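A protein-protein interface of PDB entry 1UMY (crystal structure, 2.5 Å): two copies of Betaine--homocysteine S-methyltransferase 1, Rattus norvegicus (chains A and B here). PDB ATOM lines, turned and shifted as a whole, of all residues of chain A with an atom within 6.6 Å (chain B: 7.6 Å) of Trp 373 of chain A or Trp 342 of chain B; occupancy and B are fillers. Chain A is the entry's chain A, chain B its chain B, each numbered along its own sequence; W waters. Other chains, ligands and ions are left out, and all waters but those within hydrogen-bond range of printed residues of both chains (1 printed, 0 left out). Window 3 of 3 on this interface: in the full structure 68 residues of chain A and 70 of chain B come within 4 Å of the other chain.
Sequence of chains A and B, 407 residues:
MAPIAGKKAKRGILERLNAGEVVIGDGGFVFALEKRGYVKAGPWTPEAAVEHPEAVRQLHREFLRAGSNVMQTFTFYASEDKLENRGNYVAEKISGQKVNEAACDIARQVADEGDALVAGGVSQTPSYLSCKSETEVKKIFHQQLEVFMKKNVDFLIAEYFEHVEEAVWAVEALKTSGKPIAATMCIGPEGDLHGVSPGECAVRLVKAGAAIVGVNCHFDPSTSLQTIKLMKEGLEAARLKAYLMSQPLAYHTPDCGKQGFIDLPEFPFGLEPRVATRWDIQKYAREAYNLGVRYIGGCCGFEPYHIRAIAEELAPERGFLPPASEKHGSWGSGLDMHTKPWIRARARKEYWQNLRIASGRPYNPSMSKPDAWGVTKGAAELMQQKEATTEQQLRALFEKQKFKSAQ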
ATOM      1  N   GLN A 259      -3.754 -19.731  -2.159  1.00  0.00           N
ATOM      2  CA  GLN A 259      -4.656 -20.863  -2.228  1.00  0.00           C
ATOM      3  C   GLN A 259      -4.106 -21.687  -3.395  1.00  0.00           C
ATOM      4  O   GLN A 259      -4.487 -21.547  -4.558  1.00  0.00           O
ATOM      5  CB  GLN A 259      -6.119 -20.443  -2.473  1.00  0.00           C
ATOM      6  CG  GLN A 259      -7.077 -21.635  -2.783  1.00  0.00           C
ATOM      7  CD  GLN A 259      -7.386 -22.539  -1.579  1.00  0.00           C
ATOM      8  OE1 GLN A 259      -8.084 -22.136  -0.634  1.00  0.00           O
ATOM      9  NE2 GLN A 259      -6.874 -23.767  -1.618  1.00  0.00           N
ATOM     10  N   ILE A 262      -4.393 -25.282  -6.781  1.00  0.00           N
ATOM     11  CA  ILE A 262      -5.766 -25.645  -7.078  1.00  0.00           C
ATOM     12  C   ILE A 262      -6.492 -24.507  -7.773  1.00  0.00           C
ATOM     13  O   ILE A 262      -7.398 -24.735  -8.549  1.00  0.00           O
ATOM     14  CB  ILE A 262      -6.490 -26.052  -5.791  1.00  0.00           C
ATOM     15  CG1 ILE A 262      -6.404 -27.571  -5.635  1.00  0.00           C
ATOM     16  CG2 ILE A 262      -7.916 -25.548  -5.789  1.00  0.00           C
ATOM     17  CD1 ILE A 262      -6.742 -28.045  -4.245  1.00  0.00           C
ATOM     18  N   ASP A 263      -6.082 -23.279  -7.492  1.00  0.00           N
ATOM     19  CA  ASP A 263      -6.674 -22.103  -8.134  1.00  0.00           C
ATOM     20  C   ASP A 263      -6.104 -21.896  -9.531  1.00  0.00           C
ATOM     21  O   ASP A 263      -6.614 -21.096 -10.302  1.00  0.00           O
ATOM     22  CB  ASP A 263      -6.406 -20.855  -7.306  1.00  0.00           C
ATOM     23  CG  ASP A 263      -7.324 -20.741  -6.121  1.00  0.00           C
ATOM     24  OD1 ASP A 263      -7.813 -21.776  -5.631  1.00  0.00           O
ATOM     25  OD2 ASP A 263      -7.551 -19.609  -5.668  1.00  0.00           O
ATOM     26  N   LEU A 264      -5.034 -22.610  -9.850  1.00  0.00           N
ATOM     27  CA  LEU A 264      -4.425 -22.494 -11.159  1.00  0.00           C
ATOM     28  C   LEU A 264      -5.322 -23.097 -12.237  1.00  0.00           C
ATOM     29  O   LEU A 264      -5.917 -24.155 -12.061  1.00  0.00           O
ATOM     30  CB  LEU A 264      -3.042 -23.155 -11.163  1.00  0.00           C
ATOM     31  CG  LEU A 264      -1.936 -22.446 -10.362  1.00  0.00           C
ATOM     32  CD1 LEU A 264      -0.673 -23.282 -10.352  1.00  0.00           C
ATOM     33  CD2 LEU A 264      -1.663 -21.089 -10.962  1.00  0.00           C
ATOM     34  N   ASP A 371      -7.326 -18.443 -10.656  1.00  0.00           N
ATOM     35  CA  ASP A 371      -8.761 -18.223 -10.867  1.00  0.00           C
ATOM     36  C   ASP A 371      -9.455 -17.506  -9.714  1.00  0.00           C
ATOM     37  O   ASP A 371     -10.416 -16.763  -9.939  1.00  0.00           O
ATOM     38  CB  ASP A 371      -9.456 -19.564 -11.113  1.00  0.00           C
ATOM     39  CG  ASP A 371      -9.730 -19.817 -12.581  1.00  0.00           C
ATOM     40  OD1 ASP A 371      -9.934 -20.984 -12.990  1.00  0.00           O
ATOM     41  OD2 ASP A 371      -9.753 -18.828 -13.337  1.00  0.00           O
ATOM     42  N   ALA A 372      -8.969 -17.769  -8.493  1.00  0.00           N
ATOM     43  CA  ALA A 372      -9.473 -17.215  -7.218  1.00  0.00           C
ATOM     44  C   ALA A 372     -10.344 -15.955  -7.300  1.00  0.00           C
ATOM     45  O   ALA A 372      -9.832 -14.851  -7.477  1.00  0.00           O
ATOM     46  CB  ALA A 372      -8.287 -16.959  -6.258  1.00  0.00           C
ATOM     47  N   TRP A 373     -11.651 -16.123  -7.134  1.00  0.00           N
ATOM     48  CA  TRP A 373     -12.579 -15.002  -7.217  1.00  0.00           C
ATOM     49  C   TRP A 373     -12.562 -14.009  -6.068  1.00  0.00           C
ATOM     50  O   TRP A 373     -12.678 -14.382  -4.895  1.00  0.00           O
ATOM     51  CB  TRP A 373     -14.009 -15.517  -7.421  1.00  0.00           C
ATOM     52  CG  TRP A 373     -14.405 -15.462  -8.859  1.00  0.00           C
ATOM     53  CD1 TRP A 373     -13.861 -16.187  -9.897  1.00  0.00           C
ATOM     54  CD2 TRP A 373     -15.322 -14.542  -9.449  1.00  0.00           C
ATOM     55  NE1 TRP A 373     -14.380 -15.760 -11.093  1.00  0.00           N
ATOM     56  CE2 TRP A 373     -15.281 -14.752 -10.852  1.00  0.00           C
ATOM     57  CE3 TRP A 373     -16.174 -13.551  -8.934  1.00  0.00           C
ATOM     58  CZ2 TRP A 373     -16.064 -14.006 -11.746  1.00  0.00           C
ATOM     59  CZ3 TRP A 373     -16.951 -12.809  -9.824  1.00  0.00           C
ATOM     60  CH2 TRP A 373     -16.889 -13.043 -11.217  1.00  0.00           C
ATOM     61  N   GLY A 374     -12.440 -12.730  -6.420  1.00  0.00           N
ATOM     62  CA  GLY A 374     -12.407 -11.693  -5.408  1.00  0.00           C
ATOM     63  C   GLY A 374     -13.500 -10.651  -5.580  1.00  0.00           C
ATOM     64  O   GLY A 374     -14.320 -10.447  -4.663  1.00  0.00           O
ATOM     65  N   VAL A 375     -13.530 -10.003  -6.748  1.00  0.00           N
ATOM     66  CA  VAL A 375     -14.522  -8.968  -7.001  1.00  0.00           C
ATOM     67  C   VAL A 375     -15.382  -9.020  -8.265  1.00  0.00           C
ATOM     68  O   VAL A 375     -15.095  -9.711  -9.253  1.00  0.00           O
ATOM     69  CB  VAL A 375     -13.886  -7.553  -6.936  1.00  0.00           C
ATOM     70  CG1 VAL A 375     -13.687  -7.138  -5.483  1.00  0.00           C
ATOM     71  CG2 VAL A 375     -12.572  -7.543  -7.693  1.00  0.00           C
ATOM     72  N   THR A 376     -16.454  -8.240  -8.180  1.00  0.00           N
ATOM     73  CA  THR A 376     -17.472  -8.063  -9.201  1.00  0.00           C
ATOM     74  C   THR A 376     -18.463  -7.081  -8.555  1.00  0.00           C
ATOM     75  O   THR A 376     -19.399  -6.592  -9.200  1.00  0.00           O
ATOM     76  CB  THR A 376     -18.197  -9.386  -9.534  1.00  0.00           C
ATOM     77  OG1 THR A 376     -19.503  -9.096 -10.065  1.00  0.00           O
ATOM     78  CG2 THR A 376     -18.326 -10.259  -8.281  1.00  0.00           C
ATOM     79  N   ALA A 380     -14.999  -4.394 -10.728  1.00  0.00           N
ATOM     80  CA  ALA A 380     -15.342  -5.326 -11.810  1.00  0.00           C
ATOM     81  C   ALA A 380     -16.150  -4.567 -12.855  1.00  0.00           C
ATOM     82  O   ALA A 380     -15.619  -4.160 -13.890  1.00  0.00           O
ATOM     83  CB  ALA A 380     -16.144  -6.495 -11.272  1.00  0.00           C
ATOM     84  N   LEU B 335     -15.256 -32.935 -11.910  1.00  0.00           N
ATOM     85  CA  LEU B 335     -15.084 -31.653 -11.253  1.00  0.00           C
ATOM     86  C   LEU B 335     -16.422 -30.950 -11.057  1.00  0.00           C
ATOM     87  O   LEU B 335     -16.454 -29.839 -10.536  1.00  0.00           O
ATOM     88  CB  LEU B 335     -14.148 -30.768 -12.073  1.00  0.00           C
ATOM     89  CG  LEU B 335     -12.633 -30.885 -11.860  1.00  0.00           C
ATOM     90  CD1 LEU B 335     -12.171 -32.310 -11.938  1.00  0.00           C
ATOM     91  CD2 LEU B 335     -11.943 -30.038 -12.904  1.00  0.00           C
ATOM     92  N   HIS B 338     -17.429 -30.009  -6.077  1.00  0.00           N
ATOM     93  CA  HIS B 338     -16.307 -29.171  -5.631  1.00  0.00           C
ATOM     94  C   HIS B 338     -16.822 -27.797  -5.257  1.00  0.00           C
ATOM     95  O   HIS B 338     -17.183 -27.009  -6.115  1.00  0.00           O
ATOM     96  CB  HIS B 338     -15.227 -29.029  -6.702  1.00  0.00           C
ATOM     97  CG  HIS B 338     -13.920 -28.544  -6.167  1.00  0.00           C
ATOM     98  ND1 HIS B 338     -13.760 -27.286  -5.628  1.00  0.00           N
ATOM     99  CD2 HIS B 338     -12.732 -29.174  -6.020  1.00  0.00           C
ATOM    100  CE1 HIS B 338     -12.529 -27.166  -5.164  1.00  0.00           C
ATOM    101  NE2 HIS B 338     -11.886 -28.297  -5.389  1.00  0.00           N
ATOM    102  N   THR B 339     -16.848 -27.534  -3.959  1.00  0.00           N
ATOM    103  CA  THR B 339     -17.336 -26.289  -3.391  1.00  0.00           C
ATOM    104  C   THR B 339     -16.961 -25.037  -4.162  1.00  0.00           C
ATOM    105  O   THR B 339     -17.682 -24.037  -4.120  1.00  0.00           O
ATOM    106  CB  THR B 339     -16.841 -26.153  -1.951  1.00  0.00           C
ATOM    107  OG1 THR B 339     -15.410 -26.117  -1.939  1.00  0.00           O
ATOM    108  CG2 THR B 339     -17.295 -27.361  -1.127  1.00  0.00           C
ATOM    109  N   LYS B 340     -15.838 -25.093  -4.869  1.00  0.00           N
ATOM    110  CA  LYS B 340     -15.369 -23.948  -5.641  1.00  0.00           C
ATOM    111  C   LYS B 340     -16.010 -23.868  -7.018  1.00  0.00           C
ATOM    112  O   LYS B 340     -15.990 -24.818  -7.790  1.00  0.00           O
ATOM    113  CB  LYS B 340     -13.842 -23.994  -5.776  1.00  0.00           C
ATOM    114  CG  LYS B 340     -13.110 -23.939  -4.436  1.00  0.00           C
ATOM    115  CD  LYS B 340     -13.349 -22.613  -3.720  1.00  0.00           C
ATOM    116  CE  LYS B 340     -13.636 -22.794  -2.217  1.00  0.00           C
ATOM    117  NZ  LYS B 340     -12.473 -23.253  -1.390  1.00  0.00           N
ATOM    118  N   PRO B 341     -16.599 -22.716  -7.336  1.00  0.00           N
ATOM    119  CA  PRO B 341     -17.269 -22.456  -8.607  1.00  0.00           C
ATOM    120  C   PRO B 341     -16.327 -22.420  -9.804  1.00  0.00           C
ATOM    121  O   PRO B 341     -16.608 -22.997 -10.855  1.00  0.00           O
ATOM    122  CB  PRO B 341     -17.934 -21.097  -8.366  1.00  0.00           C
ATOM    123  CG  PRO B 341     -18.182 -21.094  -6.897  1.00  0.00           C
ATOM    124  CD  PRO B 341     -16.881 -21.636  -6.375  1.00  0.00           C
ATOM    125  N   TRP B 342     -15.211 -21.723  -9.642  1.00  0.00           N
ATOM    126  CA  TRP B 342     -14.247 -21.604 -10.722  1.00  0.00           C
ATOM    127  C   TRP B 342     -13.623 -22.952 -11.084  1.00  0.00           C
ATOM    128  O   TRP B 342     -13.230 -23.175 -12.238  1.00  0.00           O
ATOM    129  CB  TRP B 342     -13.176 -20.570 -10.361  1.00  0.00           C
ATOM    130  CG  TRP B 342     -12.475 -20.798  -9.067  1.00  0.00           C
ATOM    131  CD1 TRP B 342     -11.391 -21.597  -8.849  1.00  0.00           C
ATOM    132  CD2 TRP B 342     -12.777 -20.181  -7.813  1.00  0.00           C
ATOM    133  NE1 TRP B 342     -10.991 -21.509  -7.536  1.00  0.00           N
ATOM    134  CE2 TRP B 342     -11.825 -20.646  -6.877  1.00  0.00           C
ATOM    135  CE3 TRP B 342     -13.761 -19.278  -7.386  1.00  0.00           C
ATOM    136  CZ2 TRP B 342     -11.827 -20.237  -5.539  1.00  0.00           C
ATOM    137  CZ3 TRP B 342     -13.764 -18.875  -6.053  1.00  0.00           C
ATOM    138  CH2 TRP B 342     -12.802 -19.356  -5.147  1.00  0.00           C
ATOM    139  N   ILE B 343     -13.553 -23.853 -10.110  1.00  0.00           N
ATOM    140  CA  ILE B 343     -13.009 -25.166 -10.381  1.00  0.00           C
ATOM    141  C   ILE B 343     -14.072 -26.017 -11.064  1.00  0.00           C
ATOM    142  O   ILE B 343     -13.763 -26.816 -11.945  1.00  0.00           O
ATOM    143  CB  ILE B 343     -12.536 -25.858  -9.094  1.00  0.00           C
ATOM    144  CG1 ILE B 343     -11.253 -25.184  -8.603  1.00  0.00           C
ATOM    145  CG2 ILE B 343     -12.314 -27.340  -9.343  1.00  0.00           C
ATOM    146  CD1 ILE B 343     -10.681 -25.775  -7.341  1.00  0.00           C
ATOM    147  N   ARG B 344     -15.329 -25.841 -10.670  1.00  0.00           N
ATOM    148  CA  ARG B 344     -16.416 -26.598 -11.275  1.00  0.00           C
ATOM    149  C   ARG B 344     -16.611 -26.122 -12.710  1.00  0.00           C
ATOM    150  O   ARG B 344     -17.043 -26.870 -13.583  1.00  0.00           O
ATOM    151  CB  ARG B 344     -17.724 -26.404 -10.497  1.00  0.00           C
ATOM    152  CG  ARG B 344     -17.756 -26.972  -9.079  1.00  0.00           C
ATOM    153  CD  ARG B 344     -19.201 -27.019  -8.541  1.00  0.00           C
ATOM    154  NE  ARG B 344     -19.854 -25.711  -8.553  1.00  0.00           N
ATOM    155  CZ  ARG B 344     -19.744 -24.799  -7.591  1.00  0.00           C
ATOM    156  NH1 ARG B 344     -19.013 -25.042  -6.512  1.00  0.00           N
ATOM    157  NH2 ARG B 344     -20.354 -23.625  -7.718  1.00  0.00           N
ATOM    158  N   ALA B 345     -16.293 -24.866 -12.960  1.00  0.00           N
ATOM    159  CA  ALA B 345     -16.462 -24.334 -14.291  1.00  0.00           C
ATOM    160  C   ALA B 345     -15.441 -24.917 -15.263  1.00  0.00           C
ATOM    161  O   ALA B 345     -15.460 -24.608 -16.453  1.00  0.00           O
ATOM    162  CB  ALA B 345     -16.343 -22.828 -14.259  1.00  0.00           C
ATOM    163  N   ARG B 346     -14.543 -25.759 -14.767  1.00  0.00           N
ATOM    164  CA  ARG B 346     -13.531 -26.340 -15.636  1.00  0.00           C
ATOM    165  C   ARG B 346     -13.954 -27.699 -16.189  1.00  0.00           C
ATOM    166  O   ARG B 346     -13.279 -28.270 -17.042  1.00  0.00           O
ATOM    167  CB  ARG B 346     -12.219 -26.477 -14.878  1.00  0.00           C
ATOM    168  CG  ARG B 346     -11.636 -25.170 -14.400  1.00  0.00           C
ATOM    169  CD  ARG B 346     -10.397 -25.403 -13.536  1.00  0.00           C
ATOM    170  NE  ARG B 346      -9.931 -24.182 -12.881  1.00  0.00           N
ATOM    171  CZ  ARG B 346      -9.105 -24.159 -11.840  1.00  0.00           C
ATOM    172  NH1 ARG B 346      -8.648 -25.291 -11.335  1.00  0.00           N
ATOM    173  NH2 ARG B 346      -8.742 -23.008 -11.298  1.00  0.00           N
ATOM    174  N   ALA B 347     -15.086 -28.205 -15.705  1.00  0.00           N
ATOM    175  CA  ALA B 347     -15.592 -29.505 -16.132  1.00  0.00           C
ATOM    176  C   ALA B 347     -16.250 -29.376 -17.486  1.00  0.00           C
ATOM    177  O   ALA B 347     -17.403 -29.730 -17.656  1.00  0.00           O
ATOM    178  CB  ALA B 347     -16.591 -30.039 -15.111  1.00  0.00           C
ATOM    179  N   TYR B 351     -13.405 -25.890 -22.246  1.00  0.00           N
ATOM    180  CA  TYR B 351     -12.370 -25.316 -21.395  1.00  0.00           C
ATOM    181  C   TYR B 351     -11.009 -26.011 -21.540  1.00  0.00           C
ATOM    182  O   TYR B 351      -9.996 -25.356 -21.758  1.00  0.00           O
ATOM    183  CB  TYR B 351     -12.815 -25.359 -19.930  1.00  0.00           C
ATOM    184  CG  TYR B 351     -11.741 -24.942 -18.935  1.00  0.00           C
ATOM    185  CD1 TYR B 351     -10.743 -25.837 -18.531  1.00  0.00           C
ATOM    186  CD2 TYR B 351     -11.721 -23.652 -18.404  1.00  0.00           C
ATOM    187  CE1 TYR B 351      -9.759 -25.449 -17.629  1.00  0.00           C
ATOM    188  CE2 TYR B 351     -10.746 -23.261 -17.509  1.00  0.00           C
ATOM    189  CZ  TYR B 351      -9.768 -24.155 -17.124  1.00  0.00           C
ATOM    190  OH  TYR B 351      -8.797 -23.746 -16.237  1.00  0.00           O
HETATM  191  O   HOH W   1     -10.199 -22.408  -3.662  1.00  0.00           O
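Trp 373 of chain A touches just one residue of chain B: Trp 342 (3.6 Å).
Trp 342 of chain B touches three residues of chain A.
Of the printed residues of chain B, Leu 264 of chain A touches Arg 346.
Of the printed residues of chain B, Ile 262 of chain A touches Ile 343 (3.2 Å) and Arg 346 (3.1 Å).
Printed residues of chain A within 4 Å of Ile 343 of chain B: Ile 262.
Printed residues of chain B within 4 Å of Asp 371 of chain A: Trp 342 and Arg 346.
The nearest printed residue of chain B that does not touch Asp 263 of chain A is Ile 343 of chain B (5.2 Å).
The backbone carbonyl oxygen of Ile 262 of chain A lies within hydrogen-bond range of the guanidinium group of Arg 346 of chain B (3.1 Å).
The guanidinium group (NH2) of Arg 346 of chain B is in hydrogen-bond range of the backbone carbonyl oxygen (O) of Asp 263 of chain A (3.0 Å).
O of Leu 264 of chain A is in hydrogen-bond range of NH1 of Arg 346 of chain B, 3.0 Å away.
The guanidinium group (NH2) of Arg 346 of chain B is in salt-bridge range of the side-chain carboxylate (OD1) of Asp 371 of chain A.
No position is printed for both chains.
Among the printed residues, merely in contact across the chains: Ile 262 of chain A with Ile 343 of chain B, Asp 371 of chain A with Trp 342 of chain B, Trp 373 of chain A with Trp 342 of chain B and Asp 263 of chain A with Trp 342 of chain B.
Water W1 bridges the side-chain carboxylate (OD1) of Asp 263 of chain A (3.2 Å) and the side-chain amino group (NZ) of Lys 340 of chain B (3.3 Å).
Hydrophobic or aromatic side chains of chain B within 4 Å of the printed part of chain A: Trp 342 and Ile 343.
Hydrophobic or aromatic side chains of chain A within 4 Å of the printed part of chain B: Ile 262 and Trp 373.
Among the printed residues, 8 pairs touch across the chains.
N of Asp 371 of chain A is in hydrogen-bond range of O of Asp 263 of chain A.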
